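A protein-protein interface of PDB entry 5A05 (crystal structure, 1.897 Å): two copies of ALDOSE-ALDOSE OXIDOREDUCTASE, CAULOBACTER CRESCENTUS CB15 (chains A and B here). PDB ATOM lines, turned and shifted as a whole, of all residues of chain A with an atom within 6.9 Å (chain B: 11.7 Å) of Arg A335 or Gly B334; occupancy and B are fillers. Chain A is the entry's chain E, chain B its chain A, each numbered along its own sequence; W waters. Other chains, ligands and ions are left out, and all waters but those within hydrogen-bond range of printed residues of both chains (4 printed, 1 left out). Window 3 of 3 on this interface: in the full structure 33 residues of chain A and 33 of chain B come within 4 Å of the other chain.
N of Thr B336 sits at hydrogen-bond distance from O of Gly A334 (2.9 Å).
The side-chain amide nitrogen (ND2) of Asn B206 lies within hydrogen-bond range of the backbone carbonyl oxygen (O) of Ala A207 (3.1 Å).
N of Thr A336 sits at hydrogen-bond distance from O of Gly B334.
The backbone carbonyl oxygen (O) of Ala B207 lies within hydrogen-bond range of the side-chain amide nitrogen (ND2) of Asn A206 (3.1 Å).
The side-chain hydroxyl of Thr A336 sits at hydrogen-bond distance from the side-chain amide oxygen of Asn A206 (2.6 Å).
The guanidinium group (NE) of Arg B335 is in salt-bridge range of the side-chain carboxylate (OE1) of Glu B333, at 2.5 Å.
OD1 of Asn B206 lies within hydrogen-bond range of OG1 of Thr B336.
The backbone NH (N) of Asn B226 is in hydrogen-bond range of the backbone carbonyl oxygen (O) of Val B208 (2.9 Å).
OE1 of Glu A333 lies within salt-bridge range of NE of Arg A335 (2.6 Å).
The backbone carbonyl oxygen (O) of Asn B206 lies within hydrogen-bond range of the backbone NH (N) of Gln B228, 2.9 Å away.
Among the printed residues, pairs that only touch across the chains: Asn A206 with Val B208 (3.6 Å), Ala A207 with Gln B228 (3.6 Å), Arg A335 with Gly B334 (3.7 Å), Gly A334 with Arg B335 (3.7 Å), Asn A206 with Asn B206 (3.8 Å), Asn A206 with Gln B228 (3.8 Å) and Arg A335 with Arg B335 (3.9 Å).
Of the printed residues of chain B, Arg A335 touches Gly B334 and Arg B335.
Printed residues of chain A within 4 Å of Gly B334: Arg A335 and Thr A336.
Of chain B, only Asn B206 (3.8 Å), Ala B207 (3.1 Å), Val B208 (3.6 Å) and Gln B228 (3.8 Å) come within 4 Å of Asn A206.
Ala A207 touches just these residues of chain B: Asn B206 and Gln B228.
No residue of chain B comes within 4 Å of Ala A330.
No residue of chain B comes within 4 Å of Ala A331.
Thr A336 touches just one residue of chain B: Gly B334 (2.9 Å).
No residue of chain B comes within 4 Å of Lys A338.
Of the printed residues of chain A, Gln B228 touches Asn A206 and Ala A207.
Of the printed residues of chain A, Val B208 touches Asn A206 (3.6 Å).
Printed residues of chain A within 4 Å of Arg B335: Gly A334 (3.7 Å) and Arg A335 (3.9 Å).
Of the printed residues of chain A, Thr B336 touches Gly A334.
The nearest residue of chain A that does not touch Gly B334 is Asn A206 (5.2 Å).
The nearest printed residue of chain A that does not touch Ala B207 is Thr A336 (4.7 Å).
Of the 24 printed residues of chain B, 7 touch a printed residue of chain A.
Printed residues of chain B that touch a printed residue of chain A: Asn B206, Ala B207, Val B208, Gln B228, Gly B334, Arg B335 and Thr B336.
Among the printed residues, 11 pairs touch across the chains.
Among the printed residues, no Asp or Glu carboxylate lies within 4 Å of a Lys or Arg side-chain nitrogen of the other chain.
Asn A206 touches its own counterpart, Asn B206.
Asn A206 touches Ala B207, and with the chains exchanged Ala A207 touches Asn B206.
Gly A334 touches Thr B336, and with the chains exchanged Thr A336 touches Gly B334.
Arg A335 touches its own counterpart, Arg B335.
14 positions are printed for both chains.
Of the 11 pairs that touch across the chains among the printed residues, 8 have their exchanged pair printed and touching as well.
Water W4 lies within hydrogen-bond range of OG1 of Thr B336 (2.7 Å) and O of Ala A207 (2.9 Å).
Water W1 lies within hydrogen-bond range of the side-chain amide oxygen of Asn B206 (2.8 Å), the side-chain amide oxygen of Asn A206 (2.8 Å), the backbone NH of Thr B336 (3.2 Å) and the backbone NH of Thr A336 (3.3 Å).
Water W2 lies within hydrogen-bond range of N of Ala B207, O of Ala B330, ND2 of Asn A206 and O of Arg B335.
Water W3 lies within hydrogen-bond range of the backbone carbonyl oxygen of Ala A330, the backbone NH of Ala A207, the side-chain amide nitrogen of Asn B206 and the backbone carbonyl oxygen of Arg A335.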
ATOM      1  N   VAL A 205     -32.782   9.164 -17.257  1.00  0.00           N
ATOM      2  CA  VAL A 205     -32.008   8.517 -18.307  1.00  0.00           C
ATOM      3  C   VAL A 205     -31.020   7.500 -17.729  1.00  0.00           C
ATOM      4  O   VAL A 205     -30.241   7.834 -16.825  1.00  0.00           O
ATOM      5  CB  VAL A 205     -31.211   9.562 -19.120  1.00  0.00           C
ATOM      6  CG1 VAL A 205     -30.349   8.891 -20.177  1.00  0.00           C
ATOM      7  CG2 VAL A 205     -32.151  10.585 -19.746  1.00  0.00           C
ATOM      8  N   ASN A 206     -31.056   6.270 -18.245  1.00  0.00           N
ATOM      9  CA  ASN A 206     -29.975   5.293 -18.040  1.00  0.00           C
ATOM     10  C   ASN A 206     -29.229   5.057 -19.346  1.00  0.00           C
ATOM     11  O   ASN A 206     -29.820   5.189 -20.414  1.00  0.00           O
ATOM     12  CB  ASN A 206     -30.513   3.939 -17.552  1.00  0.00           C
ATOM     13  CG  ASN A 206     -30.733   3.894 -16.068  1.00  0.00           C
ATOM     14  OD1 ASN A 206     -30.169   4.693 -15.317  1.00  0.00           O
ATOM     15  ND2 ASN A 206     -31.558   2.949 -15.627  1.00  0.00           N
ATOM     16  N   ALA A 207     -27.959   4.667 -19.282  1.00  0.00           N
ATOM     17  CA  ALA A 207     -27.266   4.287 -20.517  1.00  0.00           C
ATOM     18  C   ALA A 207     -26.138   3.295 -20.270  1.00  0.00           C
ATOM     19  O   ALA A 207     -25.537   3.265 -19.186  1.00  0.00           O
ATOM     20  CB  ALA A 207     -26.721   5.533 -21.244  1.00  0.00           C
ATOM     21  N   ALA A 326     -27.207  13.938 -21.377  1.00  0.00           N
ATOM     22  CA  ALA A 326     -27.549  13.131 -20.205  1.00  0.00           C
ATOM     23  C   ALA A 326     -27.290  11.637 -20.450  1.00  0.00           C
ATOM     24  O   ALA A 326     -26.922  10.921 -19.535  1.00  0.00           O
ATOM     25  CB  ALA A 326     -29.018  13.359 -19.805  1.00  0.00           C
ATOM     26  N   ARG A 329     -23.608  11.186 -20.125  1.00  0.00           N
ATOM     27  CA  ARG A 329     -23.263  11.274 -18.691  1.00  0.00           C
ATOM     28  C   ARG A 329     -23.677  10.009 -17.947  1.00  0.00           C
ATOM     29  O   ARG A 329     -22.924   9.498 -17.122  1.00  0.00           O
ATOM     30  CB  ARG A 329     -23.910  12.494 -18.033  1.00  0.00           C
ATOM     31  CG  ARG A 329     -23.513  12.677 -16.546  1.00  0.00           C
ATOM     32  CD  ARG A 329     -24.139  13.932 -15.937  1.00  0.00           C
ATOM     33  NE  ARG A 329     -23.911  15.107 -16.775  1.00  0.00           N
ATOM     34  CZ  ARG A 329     -24.866  15.754 -17.450  1.00  0.00           C
ATOM     35  NH1 ARG A 329     -26.138  15.361 -17.372  1.00  0.00           N
ATOM     36  NH2 ARG A 329     -24.550  16.807 -18.202  1.00  0.00           N
ATOM     37  N   ALA A 330     -24.867   9.490 -18.259  1.00  0.00           N
ATOM     38  CA  ALA A 330     -25.378   8.307 -17.564  1.00  0.00           C
ATOM     39  C   ALA A 330     -24.482   7.114 -17.812  1.00  0.00           C
ATOM     40  O   ALA A 330     -24.250   6.305 -16.914  1.00  0.00           O
ATOM     41  CB  ALA A 330     -26.813   7.991 -18.001  1.00  0.00           C
ATOM     42  N   ALA A 331     -23.979   7.004 -19.036  1.00  0.00           N
ATOM     43  CA  ALA A 331     -23.049   5.931 -19.392  1.00  0.00           C
ATOM     44  C   ALA A 331     -21.708   6.102 -18.680  1.00  0.00           C
ATOM     45  O   ALA A 331     -21.119   5.146 -18.189  1.00  0.00           O
ATOM     46  CB  ALA A 331     -22.836   5.896 -20.912  1.00  0.00           C
ATOM     47  N   ARG A 332     -21.229   7.338 -18.648  1.00  0.00           N
ATOM     48  CA  ARG A 332     -19.930   7.652 -18.064  1.00  0.00           C
ATOM     49  C   ARG A 332     -19.959   7.419 -16.563  1.00  0.00           C
ATOM     50  O   ARG A 332     -19.046   6.816 -16.004  1.00  0.00           O
ATOM     51  CB  ARG A 332     -19.554   9.108 -18.390  1.00  0.00           C
ATOM     52  CG  ARG A 332     -18.197   9.578 -17.886  1.00  0.00           C
ATOM     53  CD  ARG A 332     -17.833  10.909 -18.538  1.00  0.00           C
ATOM     54  NE  ARG A 332     -18.806  11.978 -18.268  1.00  0.00           N
ATOM     55  CZ  ARG A 332     -19.526  12.601 -19.204  1.00  0.00           C
ATOM     56  NH1 ARG A 332     -19.395  12.274 -20.491  1.00  0.00           N
ATOM     57  NH2 ARG A 332     -20.373  13.569 -18.859  1.00  0.00           N
ATOM     58  N   GLU A 333     -21.027   7.869 -15.907  1.00  0.00           N
ATOM     59  CA  GLU A 333     -21.077   7.810 -14.454  1.00  0.00           C
ATOM     60  C   GLU A 333     -21.785   6.568 -13.908  1.00  0.00           C
ATOM     61  O   GLU A 333     -21.776   6.325 -12.709  1.00  0.00           O
ATOM     62  CB  GLU A 333     -21.736   9.080 -13.917  1.00  0.00           C
ATOM     63  CG  GLU A 333     -20.851  10.315 -14.153  1.00  0.00           C
ATOM     64  CD  GLU A 333     -21.472  11.600 -13.646  1.00  0.00           C
ATOM     65  OE1 GLU A 333     -22.452  11.521 -12.881  1.00  0.00           O
ATOM     66  OE2 GLU A 333     -20.979  12.689 -14.021  1.00  0.00           O
ATOM     67  N   GLY A 334     -22.394   5.780 -14.788  1.00  0.00           N
ATOM     68  CA  GLY A 334     -23.059   4.565 -14.358  1.00  0.00           C
ATOM     69  C   GLY A 334     -24.176   4.832 -13.362  1.00  0.00           C
ATOM     70  O   GLY A 334     -24.284   4.161 -12.333  1.00  0.00           O
ATOM     71  N   ARG A 335     -25.014   5.819 -13.658  1.00  0.00           N
ATOM     72  CA  ARG A 335     -26.125   6.139 -12.772  1.00  0.00           C
ATOM     73  C   ARG A 335     -27.276   6.709 -13.579  1.00  0.00           C
ATOM     74  O   ARG A 335     -27.099   7.135 -14.725  1.00  0.00           O
ATOM     75  CB  ARG A 335     -25.702   7.140 -11.688  1.00  0.00           C
ATOM     76  CG  ARG A 335     -25.361   8.516 -12.243  1.00  0.00           C
ATOM     77  CD  ARG A 335     -24.965   9.532 -11.149  1.00  0.00           C
ATOM     78  NE  ARG A 335     -24.658  10.842 -11.729  1.00  0.00           N
ATOM     79  CZ  ARG A 335     -25.559  11.788 -11.986  1.00  0.00           C
ATOM     80  NH1 ARG A 335     -26.843  11.587 -11.701  1.00  0.00           N
ATOM     81  NH2 ARG A 335     -25.176  12.945 -12.525  1.00  0.00           N
ATOM     82  N   THR A 336     -28.449   6.732 -12.966  1.00  0.00           N
ATOM     83  CA  THR A 336     -29.626   7.315 -13.584  1.00  0.00           C
ATOM     84  C   THR A 336     -29.494   8.830 -13.510  1.00  0.00           C
ATOM     85  O   THR A 336     -29.331   9.388 -12.431  1.00  0.00           O
ATOM     86  CB  THR A 336     -30.917   6.854 -12.875  1.00  0.00           C
ATOM     87  OG1 THR A 336     -31.016   5.427 -12.939  1.00  0.00           O
ATOM     88  CG2 THR A 336     -32.159   7.484 -13.509  1.00  0.00           C
ATOM     89  N   VAL A 337     -29.549   9.499 -14.652  1.00  0.00           N
ATOM     90  CA  VAL A 337     -29.405  10.946 -14.666  1.00  0.00           C
ATOM     91  C   VAL A 337     -30.795  11.581 -14.745  1.00  0.00           C
ATOM     92  O   VAL A 337     -31.620  11.176 -15.555  1.00  0.00           O
ATOM     93  CB  VAL A 337     -28.492  11.399 -15.842  1.00  0.00           C
ATOM     94  CG1 VAL A 337     -28.516  12.908 -16.028  1.00  0.00           C
ATOM     95  CG2 VAL A 337     -27.068  10.902 -15.620  1.00  0.00           C
ATOM     96  N   LYS A 338     -31.059  12.555 -13.881  1.00  0.00           N
ATOM     97  CA  LYS A 338     -32.361  13.211 -13.867  1.00  0.00           C
ATOM     98  C   LYS A 338     -32.356  14.447 -14.756  1.00  0.00           C
ATOM     99  O   LYS A 338     -31.364  15.175 -14.825  1.00  0.00           O
ATOM    100  CB  LYS A 338     -32.765  13.603 -12.440  1.00  0.00           C
ATOM    101  CG  LYS A 338     -32.738  12.470 -11.440  1.00  0.00           C
ATOM    102  CD  LYS A 338     -33.588  11.300 -11.910  1.00  0.00           C
ATOM    103  CE  LYS A 338     -33.741  10.245 -10.808  1.00  0.00           C
ATOM    104  NZ  LYS A 338     -32.413   9.695 -10.367  1.00  0.00           N
ATOM    105  N   ALA B 204     -22.955  -6.117 -15.597  1.00  0.00           N
ATOM    106  CA  ALA B 204     -23.497  -4.827 -15.193  1.00  0.00           C
ATOM    107  C   ALA B 204     -24.968  -4.722 -15.582  1.00  0.00           C
ATOM    108  O   ALA B 204     -25.385  -5.241 -16.620  1.00  0.00           O
ATOM    109  CB  ALA B 204     -22.692  -3.686 -15.817  1.00  0.00           C
ATOM    110  N   VAL B 205     -25.740  -4.046 -14.738  1.00  0.00           N
ATOM    111  CA  VAL B 205     -27.191  -3.972 -14.886  1.00  0.00           C
ATOM    112  C   VAL B 205     -27.708  -2.568 -14.606  1.00  0.00           C
ATOM    113  O   VAL B 205     -27.356  -1.949 -13.586  1.00  0.00           O
ATOM    114  CB  VAL B 205     -27.906  -4.949 -13.910  1.00  0.00           C
ATOM    115  CG1 VAL B 205     -29.408  -4.828 -14.036  1.00  0.00           C
ATOM    116  CG2 VAL B 205     -27.472  -6.386 -14.166  1.00  0.00           C
ATOM    117  N   ASN B 206     -28.544  -2.072 -15.515  1.00  0.00           N
ATOM    118  CA  ASN B 206     -29.330  -0.856 -15.315  1.00  0.00           C
ATOM    119  C   ASN B 206     -30.811  -1.225 -15.280  1.00  0.00           C
ATOM    120  O   ASN B 206     -31.196  -2.188 -15.928  1.00  0.00           O
ATOM    121  CB  ASN B 206     -29.113   0.132 -16.464  1.00  0.00           C
ATOM    122  CG  ASN B 206     -27.939   1.059 -16.241  1.00  0.00           C
ATOM    123  OD1 ASN B 206     -27.449   1.228 -15.118  1.00  0.00           O
ATOM    124  ND2 ASN B 206     -27.489   1.681 -17.326  1.00  0.00           N
ATOM    125  N   ALA B 207     -31.649  -0.450 -14.597  1.00  0.00           N
ATOM    126  CA  ALA B 207     -33.094  -0.696 -14.701  1.00  0.00           C
ATOM    127  C   ALA B 207     -33.917   0.557 -14.415  1.00  0.00           C
ATOM    128  O   ALA B 207     -33.477   1.477 -13.707  1.00  0.00           O
ATOM    129  CB  ALA B 207     -33.517  -1.839 -13.767  1.00  0.00           C
ATOM    130  N   VAL B 208     -35.110   0.576 -15.001  1.00  0.00           N
ATOM    131  CA  VAL B 208     -36.103   1.628 -14.816  1.00  0.00           C
ATOM    132  C   VAL B 208     -37.410   0.948 -14.471  1.00  0.00           C
ATOM    133  O   VAL B 208     -37.845   0.073 -15.205  1.00  0.00           O
ATOM    134  CB  VAL B 208     -36.303   2.483 -16.093  1.00  0.00           C
ATOM    135  CG1 VAL B 208     -37.494   3.418 -15.911  1.00  0.00           C
ATOM    136  CG2 VAL B 208     -35.053   3.279 -16.413  1.00  0.00           C
ATOM    137  N   GLU B 209     -38.041   1.343 -13.373  1.00  0.00           N
ATOM    138  CA  GLU B 209     -39.302   0.732 -12.982  1.00  0.00           C
ATOM    139  C   GLU B 209     -40.419   1.758 -13.128  1.00  0.00           C
ATOM    140  O   GLU B 209     -40.227   2.931 -12.820  1.00  0.00           O
ATOM    141  CB  GLU B 209     -39.206   0.197 -11.547  1.00  0.00           C
ATOM    142  CG  GLU B 209     -40.475  -0.450 -11.022  1.00  0.00           C
ATOM    143  CD  GLU B 209     -41.224   0.467 -10.065  1.00  0.00           C
ATOM    144  OE1 GLU B 209     -40.562   1.090  -9.204  1.00  0.00           O
ATOM    145  OE2 GLU B 209     -42.466   0.574 -10.173  1.00  0.00           O
ATOM    146  N   ILE B 225     -40.729  -3.056 -15.513  1.00  0.00           N
ATOM    147  CA  ILE B 225     -39.357  -2.825 -15.102  1.00  0.00           C
ATOM    148  C   ILE B 225     -38.487  -3.258 -16.263  1.00  0.00           C
ATOM    149  O   ILE B 225     -38.397  -4.435 -16.601  1.00  0.00           O
ATOM    150  CB  ILE B 225     -39.011  -3.537 -13.750  1.00  0.00           C
ATOM    151  CG1 ILE B 225     -37.572  -3.232 -13.324  1.00  0.00           C
ATOM    152  CG2 ILE B 225     -39.329  -5.035 -13.785  1.00  0.00           C
ATOM    153  CD1 ILE B 225     -37.247  -3.701 -11.890  1.00  0.00           C
ATOM    154  N   ASN B 226     -37.915  -2.266 -16.932  1.00  0.00           N
ATOM    155  CA  ASN B 226     -37.087  -2.514 -18.106  1.00  0.00           C
ATOM    156  C   ASN B 226     -35.648  -2.482 -17.668  1.00  0.00           C
ATOM    157  O   ASN B 226     -35.309  -1.743 -16.751  1.00  0.00           O
ATOM    158  CB  ASN B 226     -37.333  -1.469 -19.194  1.00  0.00           C
ATOM    159  CG  ASN B 226     -38.773  -1.438 -19.640  1.00  0.00           C
ATOM    160  OD1 ASN B 226     -39.477  -2.442 -19.534  1.00  0.00           O
ATOM    161  ND2 ASN B 226     -39.233  -0.276 -20.115  1.00  0.00           N
ATOM    162  N   PHE B 227     -34.798  -3.276 -18.304  1.00  0.00           N
ATOM    163  CA  PHE B 227     -33.425  -3.330 -17.834  1.00  0.00           C
ATOM    164  C   PHE B 227     -32.418  -3.461 -18.972  1.00  0.00           C
ATOM    165  O   PHE B 227     -32.764  -3.863 -20.087  1.00  0.00           O
ATOM    166  CB  PHE B 227     -33.256  -4.470 -16.801  1.00  0.00           C
ATOM    167  CG  PHE B 227     -33.787  -5.821 -17.240  1.00  0.00           C
ATOM    168  CD1 PHE B 227     -35.147  -6.128 -17.128  1.00  0.00           C
ATOM    169  CD2 PHE B 227     -32.921  -6.803 -17.700  1.00  0.00           C
ATOM    170  CE1 PHE B 227     -35.630  -7.380 -17.493  1.00  0.00           C
ATOM    171  CE2 PHE B 227     -33.396  -8.066 -18.074  1.00  0.00           C
ATOM    172  CZ  PHE B 227     -34.754  -8.352 -17.968  1.00  0.00           C
ATOM    173  N   GLN B 228     -31.186  -3.048 -18.680  1.00  0.00           N
ATOM    174  CA  GLN B 228     -30.062  -3.187 -19.598  1.00  0.00           C
ATOM    175  C   GLN B 228     -29.023  -4.101 -18.975  1.00  0.00           C
ATOM    176  O   GLN B 228     -28.803  -4.062 -17.762  1.00  0.00           O
ATOM    177  CB  GLN B 228     -29.415  -1.839 -19.907  1.00  0.00           C
ATOM    178  CG  GLN B 228     -30.373  -0.749 -20.318  1.00  0.00           C
ATOM    179  CD  GLN B 228     -29.645   0.520 -20.671  1.00  0.00           C
ATOM    180  OE1 GLN B 228     -29.078   1.184 -19.799  1.00  0.00           O
ATOM    181  NE2 GLN B 228     -29.628   0.859 -21.956  1.00  0.00           N
ATOM    182  N   GLU B 325     -32.259  -9.993  -8.721  1.00  0.00           N
ATOM    183  CA  GLU B 325     -31.956  -9.182  -7.535  1.00  0.00           C
ATOM    184  C   GLU B 325     -31.235  -7.875  -7.908  1.00  0.00           C
ATOM    185  O   GLU B 325     -31.546  -6.805  -7.368  1.00  0.00           O
ATOM    186  CB  GLU B 325     -31.109  -9.980  -6.516  1.00  0.00           C
ATOM    187  CG  GLU B 325     -31.877 -11.152  -5.891  1.00  0.00           C
ATOM    188  CD  GLU B 325     -31.276 -11.658  -4.574  1.00  0.00           C
ATOM    189  OE1 GLU B 325     -30.147 -11.224  -4.219  1.00  0.00           O
ATOM    190  OE2 GLU B 325     -31.943 -12.495  -3.909  1.00  0.00           O
ATOM    191  N   ALA B 326     -30.286  -7.961  -8.831  1.00  0.00           N
ATOM    192  CA  ALA B 326     -29.551  -6.785  -9.274  1.00  0.00           C
ATOM    193  C   ALA B 326     -30.434  -5.822 -10.062  1.00  0.00           C
ATOM    194  O   ALA B 326     -30.274  -4.607  -9.952  1.00  0.00           O
ATOM    195  CB  ALA B 326     -28.346  -7.196 -10.119  1.00  0.00           C
ATOM    196  N   ILE B 327     -31.348  -6.362 -10.870  1.00  0.00           N
ATOM    197  CA  ILE B 327     -32.292  -5.530 -11.621  1.00  0.00           C
ATOM    198  C   ILE B 327     -33.161  -4.699 -10.674  1.00  0.00           C
ATOM    199  O   ILE B 327     -33.292  -3.477 -10.828  1.00  0.00           O
ATOM    200  CB  ILE B 327     -33.183  -6.389 -12.549  1.00  0.00           C
ATOM    201  CG1 ILE B 327     -32.350  -6.915 -13.720  1.00  0.00           C
ATOM    202  CG2 ILE B 327     -34.360  -5.561 -13.067  1.00  0.00           C
ATOM    203  CD1 ILE B 327     -32.968  -8.116 -14.453  1.00  0.00           C
ATOM    204  N   TYR B 328     -33.754  -5.355  -9.684  1.00  0.00           N
ATOM    205  CA  TYR B 328     -34.561  -4.643  -8.700  1.00  0.00           C
ATOM    206  C   TYR B 328     -33.732  -3.595  -7.937  1.00  0.00           C
ATOM    207  O   TYR B 328     -34.199  -2.483  -7.694  1.00  0.00           O
ATOM    208  CB  TYR B 328     -35.180  -5.637  -7.706  1.00  0.00           C
ATOM    209  CG  TYR B 328     -36.394  -6.384  -8.219  1.00  0.00           C
ATOM    210  CD1 TYR B 328     -37.439  -5.718  -8.857  1.00  0.00           C
ATOM    211  CD2 TYR B 328     -36.510  -7.757  -8.029  1.00  0.00           C
ATOM    212  CE1 TYR B 328     -38.577  -6.425  -9.316  1.00  0.00           C
ATOM    213  CE2 TYR B 328     -37.629  -8.463  -8.474  1.00  0.00           C
ATOM    214  CZ  TYR B 328     -38.655  -7.799  -9.108  1.00  0.00           C
ATOM    215  OH  TYR B 328     -39.749  -8.518  -9.534  1.00  0.00           O
ATOM    216  N   ARG B 329     -32.503  -3.957  -7.566  1.00  0.00           N
ATOM    217  CA  ARG B 329     -31.613  -3.025  -6.870  1.00  0.00           C
ATOM    218  C   ARG B 329     -31.275  -1.820  -7.752  1.00  0.00           C
ATOM    219  O   ARG B 329     -31.253  -0.688  -7.274  1.00  0.00           O
ATOM    220  CB  ARG B 329     -30.326  -3.736  -6.421  1.00  0.00           C
ATOM    221  CG  ARG B 329     -29.380  -2.871  -5.568  1.00  0.00           C
ATOM    222  CD  ARG B 329     -28.415  -3.738  -4.740  1.00  0.00           C
ATOM    223  NE  ARG B 329     -27.712  -4.715  -5.568  1.00  0.00           N
ATOM    224  CZ  ARG B 329     -27.903  -6.037  -5.517  1.00  0.00           C
ATOM    225  NH1 ARG B 329     -28.771  -6.562  -4.650  1.00  0.00           N
ATOM    226  NH2 ARG B 329     -27.221  -6.841  -6.331  1.00  0.00           N
ATOM    227  N   ALA B 330     -31.032  -2.065  -9.042  1.00  0.00           N
ATOM    228  CA  ALA B 330     -30.641  -0.997  -9.966  1.00  0.00           C
ATOM    229  C   ALA B 330     -31.752   0.028 -10.119  1.00  0.00           C
ATOM    230  O   ALA B 330     -31.493   1.220 -10.227  1.00  0.00           O
ATOM    231  CB  ALA B 330     -30.263  -1.570 -11.325  1.00  0.00           C
ATOM    232  N   ALA B 331     -32.990  -0.449 -10.127  1.00  0.00           N
ATOM    233  CA  ALA B 331     -34.148   0.417 -10.261  1.00  0.00           C
ATOM    234  C   ALA B 331     -34.388   1.185  -8.977  1.00  0.00           C
ATOM    235  O   ALA B 331     -34.743   2.361  -9.003  1.00  0.00           O
ATOM    236  CB  ALA B 331     -35.392  -0.402 -10.629  1.00  0.00           C
ATOM    237  N   ARG B 332     -34.195   0.506  -7.850  1.00  0.00           N
ATOM    238  CA  ARG B 332     -34.378   1.128  -6.543  1.00  0.00           C
ATOM    239  C   ARG B 332     -33.327   2.208  -6.288  1.00  0.00           C
ATOM    240  O   ARG B 332     -33.639   3.292  -5.790  1.00  0.00           O
ATOM    241  CB  ARG B 332     -34.324   0.066  -5.434  1.00  0.00           C
ATOM    242  CG  ARG B 332     -34.446   0.633  -4.012  1.00  0.00           C
ATOM    243  CD  ARG B 332     -34.627  -0.475  -2.963  1.00  0.00           C
ATOM    244  NE  ARG B 332     -33.559  -1.483  -2.953  1.00  0.00           N
ATOM    245  CZ  ARG B 332     -33.716  -2.752  -3.340  1.00  0.00           C
ATOM    246  NH1 ARG B 332     -34.901  -3.177  -3.774  1.00  0.00           N
ATOM    247  NH2 ARG B 332     -32.693  -3.608  -3.289  1.00  0.00           N
ATOM    248  N   GLU B 333     -32.077   1.912  -6.623  1.00  0.00           N
ATOM    249  CA  GLU B 333     -30.978   2.823  -6.302  1.00  0.00           C
ATOM    250  C   GLU B 333     -30.622   3.784  -7.442  1.00  0.00           C
ATOM    251  O   GLU B 333     -29.846   4.714  -7.246  1.00  0.00           O
ATOM    252  CB  GLU B 333     -29.740   2.009  -5.883  1.00  0.00           C
ATOM    253  CG  GLU B 333     -30.016   1.159  -4.624  1.00  0.00           C
ATOM    254  CD  GLU B 333     -28.773   0.495  -4.040  1.00  0.00           C
ATOM    255  OE1 GLU B 333     -27.670   0.683  -4.591  1.00  0.00           O
ATOM    256  OE2 GLU B 333     -28.906  -0.219  -3.023  1.00  0.00           O
ATOM    257  N   GLY B 334     -31.183   3.559  -8.628  1.00  0.00           N
ATOM    258  CA  GLY B 334     -30.942   4.449  -9.750  1.00  0.00           C
ATOM    259  C   GLY B 334     -29.477   4.495 -10.134  1.00  0.00           C
ATOM    260  O   GLY B 334     -28.914   5.563 -10.382  1.00  0.00           O
ATOM    261  N   ARG B 335     -28.843   3.330 -10.166  1.00  0.00           N
ATOM    262  CA  ARG B 335     -27.433   3.253 -10.518  1.00  0.00           C
ATOM    263  C   ARG B 335     -27.150   1.941 -11.247  1.00  0.00           C
ATOM    264  O   ARG B 335     -27.935   0.995 -11.197  1.00  0.00           O
ATOM    265  CB  ARG B 335     -26.547   3.369  -9.264  1.00  0.00           C
ATOM    266  CG  ARG B 335     -26.581   2.136  -8.384  1.00  0.00           C
ATOM    267  CD  ARG B 335     -25.710   2.275  -7.129  1.00  0.00           C
ATOM    268  NE  ARG B 335     -25.858   1.103  -6.268  1.00  0.00           N
ATOM    269  CZ  ARG B 335     -25.169  -0.027  -6.408  1.00  0.00           C
ATOM    270  NH1 ARG B 335     -24.252  -0.144  -7.367  1.00  0.00           N
ATOM    271  NH2 ARG B 335     -25.397  -1.047  -5.583  1.00  0.00           N
ATOM    272  N   THR B 336     -26.031   1.895 -11.940  1.00  0.00           N
ATOM    273  CA  THR B 336     -25.600   0.671 -12.593  1.00  0.00           C
ATOM    274  C   THR B 336     -25.101  -0.294 -11.540  1.00  0.00           C
ATOM    275  O   THR B 336     -24.211   0.044 -10.779  1.00  0.00           O
ATOM    276  CB  THR B 336     -24.497   0.954 -13.621  1.00  0.00           C
ATOM    277  OG1 THR B 336     -24.982   1.907 -14.575  1.00  0.00           O
ATOM    278  CG2 THR B 336     -24.076  -0.341 -14.333  1.00  0.00           C
ATOM    279  N   VAL B 337     -25.685  -1.486 -11.473  1.00  0.00           N
ATOM    280  CA  VAL B 337     -25.273  -2.464 -10.474  1.00  0.00           C
ATOM    281  C   VAL B 337     -24.304  -3.466 -11.093  1.00  0.00           C
ATOM    282  O   VAL B 337     -24.566  -4.024 -12.160  1.00  0.00           O
ATOM    283  CB  VAL B 337     -26.493  -3.207  -9.861  1.00  0.00           C
ATOM    284  CG1 VAL B 337     -26.032  -4.377  -8.994  1.00  0.00           C
ATOM    285  CG2 VAL B 337     -27.343  -2.240  -9.039  1.00  0.00           C
ATOM    286  N   LYS B 338     -23.177  -3.686 -10.427  1.00  0.00           N
ATOM    287  CA  LYS B 338     -22.150  -4.579 -10.949  1.00  0.00           C
ATOM    288  C   LYS B 338     -22.296  -5.991 -10.402  1.00  0.00           C
ATOM    289  O   LYS B 338     -22.603  -6.181  -9.227  1.00  0.00           O
ATOM    290  CB  LYS B 338     -20.753  -4.040 -10.620  1.00  0.00           C
ATOM    291  CG  LYS B 338     -20.485  -2.630 -11.147  1.00  0.00           C
ATOM    292  CD  LYS B 338     -20.625  -2.549 -12.661  1.00  0.00           C
ATOM    293  CE  LYS B 338     -20.189  -1.176 -13.205  1.00  0.00           C
ATOM    294  NZ  LYS B 338     -20.869  -0.039 -12.491  1.00  0.00           N
HETATM  295  O   HOH W   1     -28.074   3.559 -13.784  1.00  0.00           O
HETATM  296  O   HOH W   2     -30.592   1.768 -12.991  1.00  0.00           O
HETATM  297  O   HOH W   3     -26.627   4.548 -16.615  1.00  0.00           O
HETATM  298  O   HOH W   4     -23.879   2.113 -17.082  1.00  0.00           O
